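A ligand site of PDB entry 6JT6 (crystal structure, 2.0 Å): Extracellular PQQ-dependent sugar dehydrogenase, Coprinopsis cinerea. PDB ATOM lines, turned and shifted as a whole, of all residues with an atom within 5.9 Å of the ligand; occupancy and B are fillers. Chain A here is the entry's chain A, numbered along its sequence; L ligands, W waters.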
ATOM      1  N   TRP A  56      -4.125 -25.751  11.733  1.00  0.00           N
ATOM      2  CA  TRP A  56      -3.521 -26.444  10.593  1.00  0.00           C
ATOM      3  C   TRP A  56      -2.145 -27.008  10.974  1.00  0.00           C
ATOM      4  O   TRP A  56      -1.559 -26.642  12.001  1.00  0.00           O
ATOM      5  CB  TRP A  56      -3.440 -25.526   9.358  1.00  0.00           C
ATOM      6  CG  TRP A  56      -2.662 -24.232   9.510  1.00  0.00           C
ATOM      7  CD1 TRP A  56      -3.172 -22.974   9.704  1.00  0.00           C
ATOM      8  CD2 TRP A  56      -1.228 -24.068   9.424  1.00  0.00           C
ATOM      9  NE1 TRP A  56      -2.140 -22.037   9.753  1.00  0.00           N
ATOM     10  CE2 TRP A  56      -0.947 -22.694   9.579  1.00  0.00           C
ATOM     11  CE3 TRP A  56      -0.146 -24.978   9.249  1.00  0.00           C
ATOM     12  CZ2 TRP A  56       0.369 -22.181   9.519  1.00  0.00           C
ATOM     13  CZ3 TRP A  56       1.165 -24.472   9.194  1.00  0.00           C
ATOM     14  CH2 TRP A  56       1.400 -23.081   9.325  1.00  0.00           C
ATOM     15  N   ILE A  57      -1.659 -27.934  10.142  1.00  0.00           N
ATOM     16  CA  ILE A  57      -0.415 -28.644  10.381  1.00  0.00           C
ATOM     17  C   ILE A  57       0.298 -28.716   9.034  1.00  0.00           C
ATOM     18  O   ILE A  57      -0.313 -29.081   8.023  1.00  0.00           O
ATOM     19  CB  ILE A  57      -0.675 -30.084  10.891  1.00  0.00           C
ATOM     20  CG1 ILE A  57      -1.695 -30.090  12.049  1.00  0.00           C
ATOM     21  CG2 ILE A  57       0.666 -30.805  11.244  1.00  0.00           C
ATOM     22  CD1 ILE A  57      -2.218 -31.489  12.414  1.00  0.00           C
ATOM     23  N   GLY A  58       1.587 -28.386   9.026  1.00  0.00           N
ATOM     24  CA  GLY A  58       2.356 -28.285   7.797  1.00  0.00           C
ATOM     25  C   GLY A  58       3.822 -28.614   7.908  1.00  0.00           C
ATOM     26  O   GLY A  58       4.338 -28.874   9.002  1.00  0.00           O
ATOM     27  N   ASN A  59       4.487 -28.680   6.759  1.00  0.00           N
ATOM     28  CA  ASN A  59       5.909 -28.972   6.746  1.00  0.00           C
ATOM     29  C   ASN A  59       6.641 -28.079   5.771  1.00  0.00           C
ATOM     30  O   ASN A  59       6.031 -27.273   5.065  1.00  0.00           O
ATOM     31  CB  ASN A  59       6.188 -30.467   6.463  1.00  0.00           C
ATOM     32  CG  ASN A  59       5.626 -30.958   5.132  1.00  0.00           C
ATOM     33  OD1 ASN A  59       5.375 -30.175   4.227  1.00  0.00           O
ATOM     34  ND2 ASN A  59       5.427 -32.267   5.021  1.00  0.00           N
ATOM     35  N   SER A  60       7.959 -28.216   5.755  1.00  0.00           N
ATOM     36  CA  SER A  60       8.791 -27.757   4.663  1.00  0.00           C
ATOM     37  C   SER A  60       9.628 -28.971   4.276  1.00  0.00           C
ATOM     38  O   SER A  60      10.239 -29.606   5.145  1.00  0.00           O
ATOM     39  CB  SER A  60       9.683 -26.615   5.099  1.00  0.00           C
ATOM     40  OG  SER A  60      10.661 -26.401   4.070  1.00  0.00           O
ATOM     41  N   GLY A  63      13.432 -28.018   4.973  1.00  0.00           N
ATOM     42  CA  GLY A  63      13.795 -27.471   6.277  1.00  0.00           C
ATOM     43  C   GLY A  63      13.366 -26.016   6.437  1.00  0.00           C
ATOM     44  O   GLY A  63      12.394 -25.705   7.143  1.00  0.00           O
ATOM     45  N   SER A  64      14.111 -25.126   5.778  1.00  0.00           N
ATOM     46  CA  SER A  64      13.792 -23.715   5.793  1.00  0.00           C
ATOM     47  C   SER A  64      12.405 -23.481   5.206  1.00  0.00           C
ATOM     48  O   SER A  64      11.990 -24.154   4.213  1.00  0.00           O
ATOM     49  CB  SER A  64      14.875 -22.945   4.977  1.00  0.00           C
ATOM     50  OG  SER A  64      14.409 -21.642   4.721  1.00  0.00           O
ATOM     51  N   MET A  65      11.674 -22.542   5.803  1.00  0.00           N
ATOM     52  CA  MET A  65      10.419 -22.073   5.233  1.00  0.00           C
ATOM     53  C   MET A  65      10.617 -21.458   3.846  1.00  0.00           C
ATOM     54  O   MET A  65       9.699 -21.464   2.991  1.00  0.00           O
ATOM     55  CB  MET A  65       9.791 -20.998   6.141  1.00  0.00           C
ATOM     56  CG  MET A  65       8.414 -20.552   5.660  1.00  0.00           C
ATOM     57  SD  MET A  65       7.737 -19.156   6.562  1.00  0.00           S
ATOM     58  CE  MET A  65       6.516 -18.708   5.317  1.00  0.00           C
ATOM     59  N   ARG A  66      11.837 -20.950   3.602  1.00  0.00           N
ATOM     60  CA  ARG A  66      12.116 -20.252   2.352  1.00  0.00           C
ATOM     61  C   ARG A  66      12.596 -21.173   1.235  1.00  0.00           C
ATOM     62  O   ARG A  66      13.603 -21.888   1.372  1.00  0.00           O
ATOM     63  CB  ARG A  66      13.108 -19.113   2.567  1.00  0.00           C
ATOM     64  CG  ARG A  66      12.590 -17.996   3.468  1.00  0.00           C
ATOM     65  CD  ARG A  66      13.757 -17.138   3.986  1.00  0.00           C
ATOM     66  NE  ARG A  66      14.789 -18.015   4.575  1.00  0.00           N
ATOM     67  CZ  ARG A  66      15.974 -18.315   4.018  1.00  0.00           C
ATOM     68  NH1 ARG A  66      16.340 -17.781   2.846  1.00  0.00           N
ATOM     69  NH2 ARG A  66      16.796 -19.160   4.638  1.00  0.00           N
ATOM     70  N   LEU A  70       6.153 -26.328   0.670  1.00  0.00           N
ATOM     71  CA  LEU A  70       5.484 -26.295   1.961  1.00  0.00           C
ATOM     72  C   LEU A  70       4.152 -27.019   1.778  1.00  0.00           C
ATOM     73  O   LEU A  70       3.355 -26.620   0.936  1.00  0.00           O
ATOM     74  CB  LEU A  70       5.276 -24.852   2.439  1.00  0.00           C
ATOM     75  CG  LEU A  70       6.469 -23.874   2.450  1.00  0.00           C
ATOM     76  CD1 LEU A  70       5.989 -22.529   2.991  1.00  0.00           C
ATOM     77  CD2 LEU A  70       7.672 -24.306   3.305  1.00  0.00           C
ATOM     78  N   LEU A  71       3.923 -28.067   2.550  1.00  0.00           N
ATOM     79  CA  LEU A  71       2.611 -28.733   2.482  1.00  0.00           C
ATOM     80  C   LEU A  71       1.849 -28.404   3.720  1.00  0.00           C
ATOM     81  O   LEU A  71       2.392 -28.433   4.817  1.00  0.00           O
ATOM     82  CB  LEU A  71       2.731 -30.254   2.285  1.00  0.00           C
ATOM     83  CG  LEU A  71       3.696 -30.771   1.219  1.00  0.00           C
ATOM     84  CD1 LEU A  71       3.693 -32.290   1.236  1.00  0.00           C
ATOM     85  CD2 LEU A  71       3.416 -30.242  -0.188  1.00  0.00           C
ATOM     86  N   VAL A  72       0.575 -28.087   3.547  1.00  0.00           N
ATOM     87  CA  VAL A  72      -0.252 -27.682   4.656  1.00  0.00           C
ATOM     88  C   VAL A  72      -1.579 -28.443   4.616  1.00  0.00           C
ATOM     89  O   VAL A  72      -2.257 -28.503   3.576  1.00  0.00           O
ATOM     90  CB  VAL A  72      -0.397 -26.146   4.759  1.00  0.00           C
ATOM     91  CG1 VAL A  72      -1.015 -25.550   3.514  1.00  0.00           C
ATOM     92  CG2 VAL A  72      -1.203 -25.737   5.987  1.00  0.00           C
ATOM     93  N   ARG A  85       2.492 -25.215  -1.058  1.00  0.00           N
ATOM     94  CA  ARG A  85       2.803 -23.779  -1.099  1.00  0.00           C
ATOM     95  C   ARG A  85       4.290 -23.474  -1.186  1.00  0.00           C
ATOM     96  O   ARG A  85       5.110 -24.379  -1.079  1.00  0.00           O
ATOM     97  CB  ARG A  85       2.159 -23.049   0.076  1.00  0.00           C
ATOM     98  CG  ARG A  85       0.693 -23.410   0.187  1.00  0.00           C
ATOM     99  CD  ARG A  85      -0.163 -22.391   0.856  1.00  0.00           C
ATOM    100  NE  ARG A  85      -1.541 -22.882   0.859  1.00  0.00           N
ATOM    101  CZ  ARG A  85      -2.571 -22.257   1.429  1.00  0.00           C
ATOM    102  NH1 ARG A  85      -2.367 -21.087   2.074  1.00  0.00           N
ATOM    103  NH2 ARG A  85      -3.786 -22.805   1.375  1.00  0.00           N
ATOM    104  N   TYR A  90       9.949 -14.863   4.794  1.00  0.00           N
ATOM    105  CA  TYR A  90       9.059 -15.057   5.955  1.00  0.00           C
ATOM    106  C   TYR A  90       7.766 -14.294   5.788  1.00  0.00           C
ATOM    107  O   TYR A  90       7.486 -13.362   6.535  1.00  0.00           O
ATOM    108  CB  TYR A  90       9.767 -14.664   7.253  1.00  0.00           C
ATOM    109  CG  TYR A  90      10.900 -15.613   7.644  1.00  0.00           C
ATOM    110  CD1 TYR A  90      10.725 -17.000   7.523  1.00  0.00           C
ATOM    111  CD2 TYR A  90      12.118 -15.135   8.141  1.00  0.00           C
ATOM    112  CE1 TYR A  90      11.719 -17.879   7.869  1.00  0.00           C
ATOM    113  CE2 TYR A  90      13.148 -16.025   8.509  1.00  0.00           C
ATOM    114  CZ  TYR A  90      12.935 -17.405   8.357  1.00  0.00           C
ATOM    115  OH  TYR A  90      13.910 -18.335   8.687  1.00  0.00           O
ATOM    116  N   ALA A  91       6.967 -14.726   4.809  1.00  0.00           N
ATOM    117  CA  ALA A  91       5.749 -14.029   4.401  1.00  0.00           C
ATOM    118  C   ALA A  91       4.674 -15.066   4.036  1.00  0.00           C
ATOM    119  O   ALA A  91       5.033 -16.214   3.802  1.00  0.00           O
ATOM    120  CB  ALA A  91       6.051 -13.149   3.203  1.00  0.00           C
ATOM    121  N   PRO A  92       3.360 -14.673   3.979  1.00  0.00           N
ATOM    122  CA  PRO A  92       2.351 -15.657   3.553  1.00  0.00           C
ATOM    123  C   PRO A  92       2.756 -16.418   2.255  1.00  0.00           C
ATOM    124  O   PRO A  92       3.042 -15.768   1.243  1.00  0.00           O
ATOM    125  CB  PRO A  92       1.083 -14.789   3.340  1.00  0.00           C
ATOM    126  CG  PRO A  92       1.264 -13.631   4.266  1.00  0.00           C
ATOM    127  CD  PRO A  92       2.741 -13.401   4.423  1.00  0.00           C
ATOM    128  N   PRO A  93       2.847 -17.758   2.312  1.00  0.00           N
ATOM    129  CA  PRO A  93       3.200 -18.526   1.096  1.00  0.00           C
ATOM    130  C   PRO A  93       2.145 -18.424  -0.005  1.00  0.00           C
ATOM    131  O   PRO A  93       0.951 -18.240   0.271  1.00  0.00           O
ATOM    132  CB  PRO A  93       3.276 -19.977   1.619  1.00  0.00           C
ATOM    133  CG  PRO A  93       3.635 -19.822   3.064  1.00  0.00           C
ATOM    134  CD  PRO A  93       2.836 -18.631   3.501  1.00  0.00           C
ATOM    135  N   GLY A 142      11.193 -29.188   7.770  1.00  0.00           N
ATOM    136  CA  GLY A 142      10.559 -28.221   8.653  1.00  0.00           C
ATOM    137  C   GLY A 142       9.219 -28.761   9.105  1.00  0.00           C
ATOM    138  O   GLY A 142       8.627 -29.677   8.469  1.00  0.00           O
ATOM    139  N   TRP A 143       8.764 -28.267  10.251  1.00  0.00           N
ATOM    140  CA  TRP A 143       7.392 -28.549  10.725  1.00  0.00           C
ATOM    141  C   TRP A 143       6.780 -27.202  11.119  1.00  0.00           C
ATOM    142  O   TRP A 143       7.497 -26.299  11.569  1.00  0.00           O
ATOM    143  CB  TRP A 143       7.392 -29.556  11.912  1.00  0.00           C
ATOM    144  CG  TRP A 143       8.185 -29.165  13.105  1.00  0.00           C
ATOM    145  CD1 TRP A 143       9.522 -29.457  13.368  1.00  0.00           C
ATOM    146  CD2 TRP A 143       7.733 -28.372  14.202  1.00  0.00           C
ATOM    147  NE1 TRP A 143       9.897 -28.914  14.569  1.00  0.00           N
ATOM    148  CE2 TRP A 143       8.830 -28.240  15.110  1.00  0.00           C
ATOM    149  CE3 TRP A 143       6.495 -27.790  14.536  1.00  0.00           C
ATOM    150  CZ2 TRP A 143       8.719 -27.539  16.340  1.00  0.00           C
ATOM    151  CZ3 TRP A 143       6.380 -27.075  15.760  1.00  0.00           C
ATOM    152  CH2 TRP A 143       7.519 -26.944  16.626  1.00  0.00           C
ATOM    153  N   ALA A 144       5.471 -27.068  10.965  1.00  0.00           N
ATOM    154  CA  ALA A 144       4.774 -25.827  11.313  1.00  0.00           C
ATOM    155  C   ALA A 144       3.361 -26.162  11.765  1.00  0.00           C
ATOM    156  O   ALA A 144       2.755 -27.157  11.296  1.00  0.00           O
ATOM    157  CB  ALA A 144       4.769 -24.827  10.131  1.00  0.00           C
ATOM    158  N   LEU A 161      -4.061 -18.257   5.221  1.00  0.00           N
ATOM    159  CA  LEU A 161      -3.896 -18.773   6.584  1.00  0.00           C
ATOM    160  C   LEU A 161      -3.080 -17.825   7.460  1.00  0.00           C
ATOM    161  O   LEU A 161      -2.281 -17.019   6.970  1.00  0.00           O
ATOM    162  CB  LEU A 161      -3.322 -20.196   6.553  1.00  0.00           C
ATOM    163  CG  LEU A 161      -2.111 -20.516   5.708  1.00  0.00           C
ATOM    164  CD1 LEU A 161      -0.885 -19.805   6.255  1.00  0.00           C
ATOM    165  CD2 LEU A 161      -1.859 -22.022   5.662  1.00  0.00           C
ATOM    166  N   TYR A 162      -3.279 -17.912   8.762  1.00  0.00           N
ATOM    167  CA  TYR A 162      -2.458 -17.167   9.716  1.00  0.00           C
ATOM    168  C   TYR A 162      -1.157 -17.908   9.927  1.00  0.00           C
ATOM    169  O   TYR A 162      -1.103 -19.142   9.870  1.00  0.00           O
ATOM    170  CB  TYR A 162      -3.204 -17.037  11.051  1.00  0.00           C
ATOM    171  CG  TYR A 162      -4.443 -16.159  10.930  1.00  0.00           C
ATOM    172  CD1 TYR A 162      -4.317 -14.761  10.771  1.00  0.00           C
ATOM    173  CD2 TYR A 162      -5.733 -16.722  10.919  1.00  0.00           C
ATOM    174  CE1 TYR A 162      -5.442 -13.951  10.630  1.00  0.00           C
ATOM    175  CE2 TYR A 162      -6.869 -15.909  10.790  1.00  0.00           C
ATOM    176  CZ  TYR A 162      -6.710 -14.532  10.636  1.00  0.00           C
ATOM    177  OH  TYR A 162      -7.824 -13.723  10.505  1.00  0.00           O
ATOM    178  N   ARG A 163      -0.098 -17.117  10.148  1.00  0.00           N
ATOM    179  CA  ARG A 163       1.196 -17.607  10.596  1.00  0.00           C
ATOM    180  C   ARG A 163       1.072 -18.638  11.715  1.00  0.00           C
ATOM    181  O   ARG A 163       0.299 -18.449  12.651  1.00  0.00           O
ATOM    182  CB  ARG A 163       2.029 -16.402  11.067  1.00  0.00           C
ATOM    183  CG  ARG A 163       3.510 -16.702  11.195  1.00  0.00           C
ATOM    184  CD  ARG A 163       4.217 -15.680  12.086  1.00  0.00           C
ATOM    185  NE  ARG A 163       4.467 -16.325  13.364  1.00  0.00           N
ATOM    186  CZ  ARG A 163       5.630 -16.893  13.716  1.00  0.00           C
ATOM    187  NH1 ARG A 163       5.745 -17.470  14.904  1.00  0.00           N
ATOM    188  NH2 ARG A 163       6.677 -16.845  12.896  1.00  0.00           N
ATOM    189  N   HIS A 164       1.840 -19.714  11.599  1.00  0.00           N
ATOM    190  CA  HIS A 164       1.946 -20.779  12.615  1.00  0.00           C
ATOM    191  C   HIS A 164       2.227 -20.196  13.995  1.00  0.00           C
ATOM    192  O   HIS A 164       2.918 -19.196  14.129  1.00  0.00           O
ATOM    193  CB  HIS A 164       3.097 -21.736  12.248  1.00  0.00           C
ATOM    194  CG  HIS A 164       4.240 -21.071  11.553  1.00  0.00           C
ATOM    195  ND1 HIS A 164       5.206 -20.363  12.239  1.00  0.00           N
ATOM    196  CD2 HIS A 164       4.570 -20.987  10.240  1.00  0.00           C
ATOM    197  CE1 HIS A 164       6.084 -19.871  11.383  1.00  0.00           C
ATOM    198  NE2 HIS A 164       5.742 -20.235  10.154  1.00  0.00           N
ATOM    199  N   HIS A 166       3.758 -22.231  16.029  1.00  0.00           N
ATOM    200  CA  HIS A 166       4.966 -23.008  16.320  1.00  0.00           C
ATOM    201  C   HIS A 166       5.568 -23.454  15.022  1.00  0.00           C
ATOM    202  O   HIS A 166       4.841 -23.903  14.118  1.00  0.00           O
ATOM    203  CB  HIS A 166       4.649 -24.280  17.141  1.00  0.00           C
ATOM    204  CG  HIS A 166       3.929 -24.040  18.439  1.00  0.00           C
ATOM    205  ND1 HIS A 166       2.577 -23.797  18.498  1.00  0.00           N
ATOM    206  CD2 HIS A 166       4.376 -24.048  19.724  1.00  0.00           C
ATOM    207  CE1 HIS A 166       2.219 -23.632  19.759  1.00  0.00           C
ATOM    208  NE2 HIS A 166       3.286 -23.789  20.523  1.00  0.00           N
ATOM    209  N   ALA A 167       6.894 -23.369  14.927  1.00  0.00           N
ATOM    210  CA  ALA A 167       7.609 -23.943  13.775  1.00  0.00           C
ATOM    211  C   ALA A 167       9.089 -24.144  14.103  1.00  0.00           C
ATOM    212  O   ALA A 167       9.666 -23.344  14.845  1.00  0.00           O
ATOM    213  CB  ALA A 167       7.449 -23.053  12.528  1.00  0.00           C
ATOM    214  N   ALA A 168       9.681 -25.211  13.583  1.00  0.00           N
ATOM    215  CA  ALA A 168      11.135 -25.401  13.637  1.00  0.00           C
ATOM    216  C   ALA A 168      11.545 -26.456  12.600  1.00  0.00           C
ATOM    217  O   ALA A 168      10.848 -26.614  11.602  1.00  0.00           O
ATOM    218  CB  ALA A 168      11.603 -25.721  15.065  1.00  0.00           C
ATOM    219  N   GLN A 169      12.694 -27.102  12.791  1.00  0.00           N
ATOM    220  CA  GLN A 169      13.283 -27.979  11.779  1.00  0.00           C
ATOM    221  C   GLN A 169      13.930 -29.120  12.500  1.00  0.00           C
ATOM    222  O   GLN A 169      14.299 -28.991  13.673  1.00  0.00           O
ATOM    223  CB  GLN A 169      14.433 -27.303  10.999  1.00  0.00           C
ATOM    224  CG  GLN A 169      14.200 -25.880  10.539  1.00  0.00           C
ATOM    225  CD  GLN A 169      15.316 -25.359   9.650  1.00  0.00           C
ATOM    226  OE1 GLN A 169      15.684 -25.981   8.640  1.00  0.00           O
ATOM    227  NE2 GLN A 169      15.828 -24.181   9.998  1.00  0.00           N
HETATM  228  C1  LIG L   1       9.560 -20.099  10.228  1.00  0.00           C
HETATM  229  C2  LIG L   1       6.582 -16.476   8.919  1.00  0.00           C
HETATM  230  C3  LIG L   1       3.439 -19.679   7.084  1.00  0.00           C
HETATM  231  C4  LIG L   1       6.835 -23.185   7.626  1.00  0.00           C
HETATM  232  C5  LIG L   1       8.996 -18.853  10.075  1.00  0.00           C
HETATM  233  C6  LIG L   1       9.523 -17.660  10.639  1.00  0.00           C
HETATM  234  C7  LIG L   1       8.665 -16.645  10.269  1.00  0.00           C
HETATM  235  C8  LIG L   1       7.616 -17.203   9.487  1.00  0.00           C
HETATM  236  C9  LIG L   1       8.801 -15.172  10.637  1.00  0.00           C
HETATM  237  C10 LIG L   1      10.787 -17.523  11.480  1.00  0.00           C
HETATM  238  C11 LIG L   1      10.707 -18.239  12.841  1.00  0.00           C
HETATM  239  C12 LIG L   1       9.494 -17.886  13.670  1.00  0.00           C
HETATM  240  O1  LIG L   1       8.585 -18.716  13.908  1.00  0.00           O
HETATM  241  O2  LIG L   1       9.407 -16.725  14.144  1.00  0.00           O
HETATM  242  C13 LIG L   1       5.456 -17.040   8.325  1.00  0.00           C
HETATM  243  C14 LIG L   1       4.316 -16.255   7.927  1.00  0.00           C
HETATM  244  C15 LIG L   1       3.398 -17.165   7.436  1.00  0.00           C
HETATM  245  C16 LIG L   1       4.031 -18.501   7.543  1.00  0.00           C
HETATM  246  C17 LIG L   1       4.171 -14.731   8.058  1.00  0.00           C
HETATM  247  C18 LIG L   1       2.030 -16.968   6.875  1.00  0.00           C
HETATM  248  C19 LIG L   1       1.179 -16.052   7.301  1.00  0.00           C
HETATM  249  C20 LIG L   1       4.125 -20.920   6.987  1.00  0.00           C
HETATM  250  C21 LIG L   1       3.591 -22.104   6.430  1.00  0.00           C
HETATM  251  C22 LIG L   1       4.554 -23.114   6.576  1.00  0.00           C
HETATM  252  C23 LIG L   1       5.686 -22.542   7.256  1.00  0.00           C
HETATM  253  C24 LIG L   1       2.228 -22.171   5.764  1.00  0.00           C
HETATM  254  C25 LIG L   1       4.434 -24.515   6.078  1.00  0.00           C
HETATM  255  C26 LIG L   1       3.255 -25.179   6.099  1.00  0.00           C
HETATM  256  C27 LIG L   1       7.812 -22.598   8.462  1.00  0.00           C
HETATM  257  C28 LIG L   1       8.979 -23.356   8.955  1.00  0.00           C
HETATM  258  C29 LIG L   1       9.745 -22.511   9.652  1.00  0.00           C
HETATM  259  C30 LIG L   1       9.032 -21.219   9.581  1.00  0.00           C
HETATM  260  C31 LIG L   1       9.293 -24.819   8.740  1.00  0.00           C
HETATM  261  C32 LIG L   1      11.026 -22.840  10.408  1.00  0.00           C
HETATM  262  C33 LIG L   1      12.284 -22.879   9.559  1.00  0.00           C
HETATM  263  C34 LIG L   1      12.669 -21.472   9.203  1.00  0.00           C
HETATM  264  O3  LIG L   1      12.709 -21.066   8.006  1.00  0.00           O
HETATM  265  O4  LIG L   1      12.908 -20.678  10.122  1.00  0.00           O
HETATM  266  N1  LIG L   1       7.813 -18.558   9.398  1.00  0.00           N
HETATM  267  N2  LIG L   1       5.246 -18.338   8.085  1.00  0.00           N
HETATM  268  N3  LIG L   1       5.366 -21.212   7.516  1.00  0.00           N
HETATM  269  N4  LIG L   1       7.900 -21.295   8.833  1.00  0.00           N
HETATM  270 FE1  LIG L   1       6.636 -19.867   8.462  1.00  0.00          FE
HETATM  271  O   HOH W   1       6.435 -20.006  14.925  1.00  0.00           O
HETATM  272  O   HOH W   2      14.519 -19.843   6.652  1.00  0.00           O
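O3 of the ligand lies within hydrogen-bond range of N of Met 65 (2.8 Å).
NH2 of Arg 163 is in salt-bridge range of O1 of the ligand (2.9 Å).
The side-chain hydroxyl (OH) of Tyr 90 lies within hydrogen-bond range of an oxygen (O4) of the ligand.
An iron atom (FE1) of the ligand is bound by the side-chain sulfur (SD) of Met 65, 2.3 Å away.
A ring nitrogen (NE2) of His 164 is bound to an iron atom (FE1) of the ligand (1.9 Å).
Water W2 lies within hydrogen-bond range of O3 of the ligand (2.6 Å), OH of Tyr 90 (2.6 Å), OG of Ser 64 (2.6 Å) and NE of Arg 66 (2.8 Å).
Water W1 lies within hydrogen-bond range of NH1 of Arg 163 (2.6 Å), O1 of the ligand (2.7 Å), ND1 of His 164 (3.0 Å) and N of Ala 167 (3.4 Å).
The backbone carbonyl oxygen (O) of Leu 71 is in hydrogen-bond range of the backbone NH (N) of Asn 59 (2.9 Å).
The side-chain hydroxyl of Ser 60 lies within hydrogen-bond range of the backbone carbonyl oxygen of Ser 64 (2.6 Å).
O of Ala 168 is in hydrogen-bond range of N of Trp 143, at 3.0 Å.
NE1 of Trp 56 lies within hydrogen-bond range of O of Tyr 162 (3.1 Å).
N of Gly 58 is in hydrogen-bond range of O of Ala 144 (2.8 Å).
The backbone NH (N) of Arg 66 lies within hydrogen-bond range of the side-chain hydroxyl (OG) of Ser 64 (2.9 Å).
N of Gly 63 lies within hydrogen-bond range of OG of Ser 60.
N of Gly 142 sits at hydrogen-bond distance from O of Ser 60, at 2.8 Å.
Trp 56 touches the ligand.
Gly 58 touches the ligand (CA to C26, 3.7 Å).
Asn 59 touches the ligand (O to C25, 3.3 Å).
Gly 63 touches the ligand (O to C31, 3.6 Å).
Ser 64 touches the ligand.
Leu 70 touches the ligand (CB to C25, 3.8 Å).
Leu 71 touches the ligand.
Pro 92 touches the ligand (CA to C18, 3.6 Å).
CD of Pro 93 touches C3 of the ligand, at 3.8 Å.
Gly 142 touches the ligand.
Trp 143 touches the ligand.
Ala 144 touches the ligand.
Leu 161 touches the ligand (O to C19, 3.6 Å).
C of Tyr 162 touches C19 of the ligand, 3.97 Å away.
Ala 167 touches the ligand.
O of Ala 168 touches C31 of the ligand, at 3.7 Å.
Gln 169 touches the ligand.
21 residues have an atom within 4 Å of the ligand: Trp 56, Gly 58, Asn 59, Gly 63, Ser 64, Met 65, Leu 70, Leu 71, Tyr 90, Pro 92, Pro 93, Gly 142, Trp 143, Ala 144, Leu 161, Tyr 162, Arg 163, His 164, Ala 167, Ala 168 and Gln 169.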
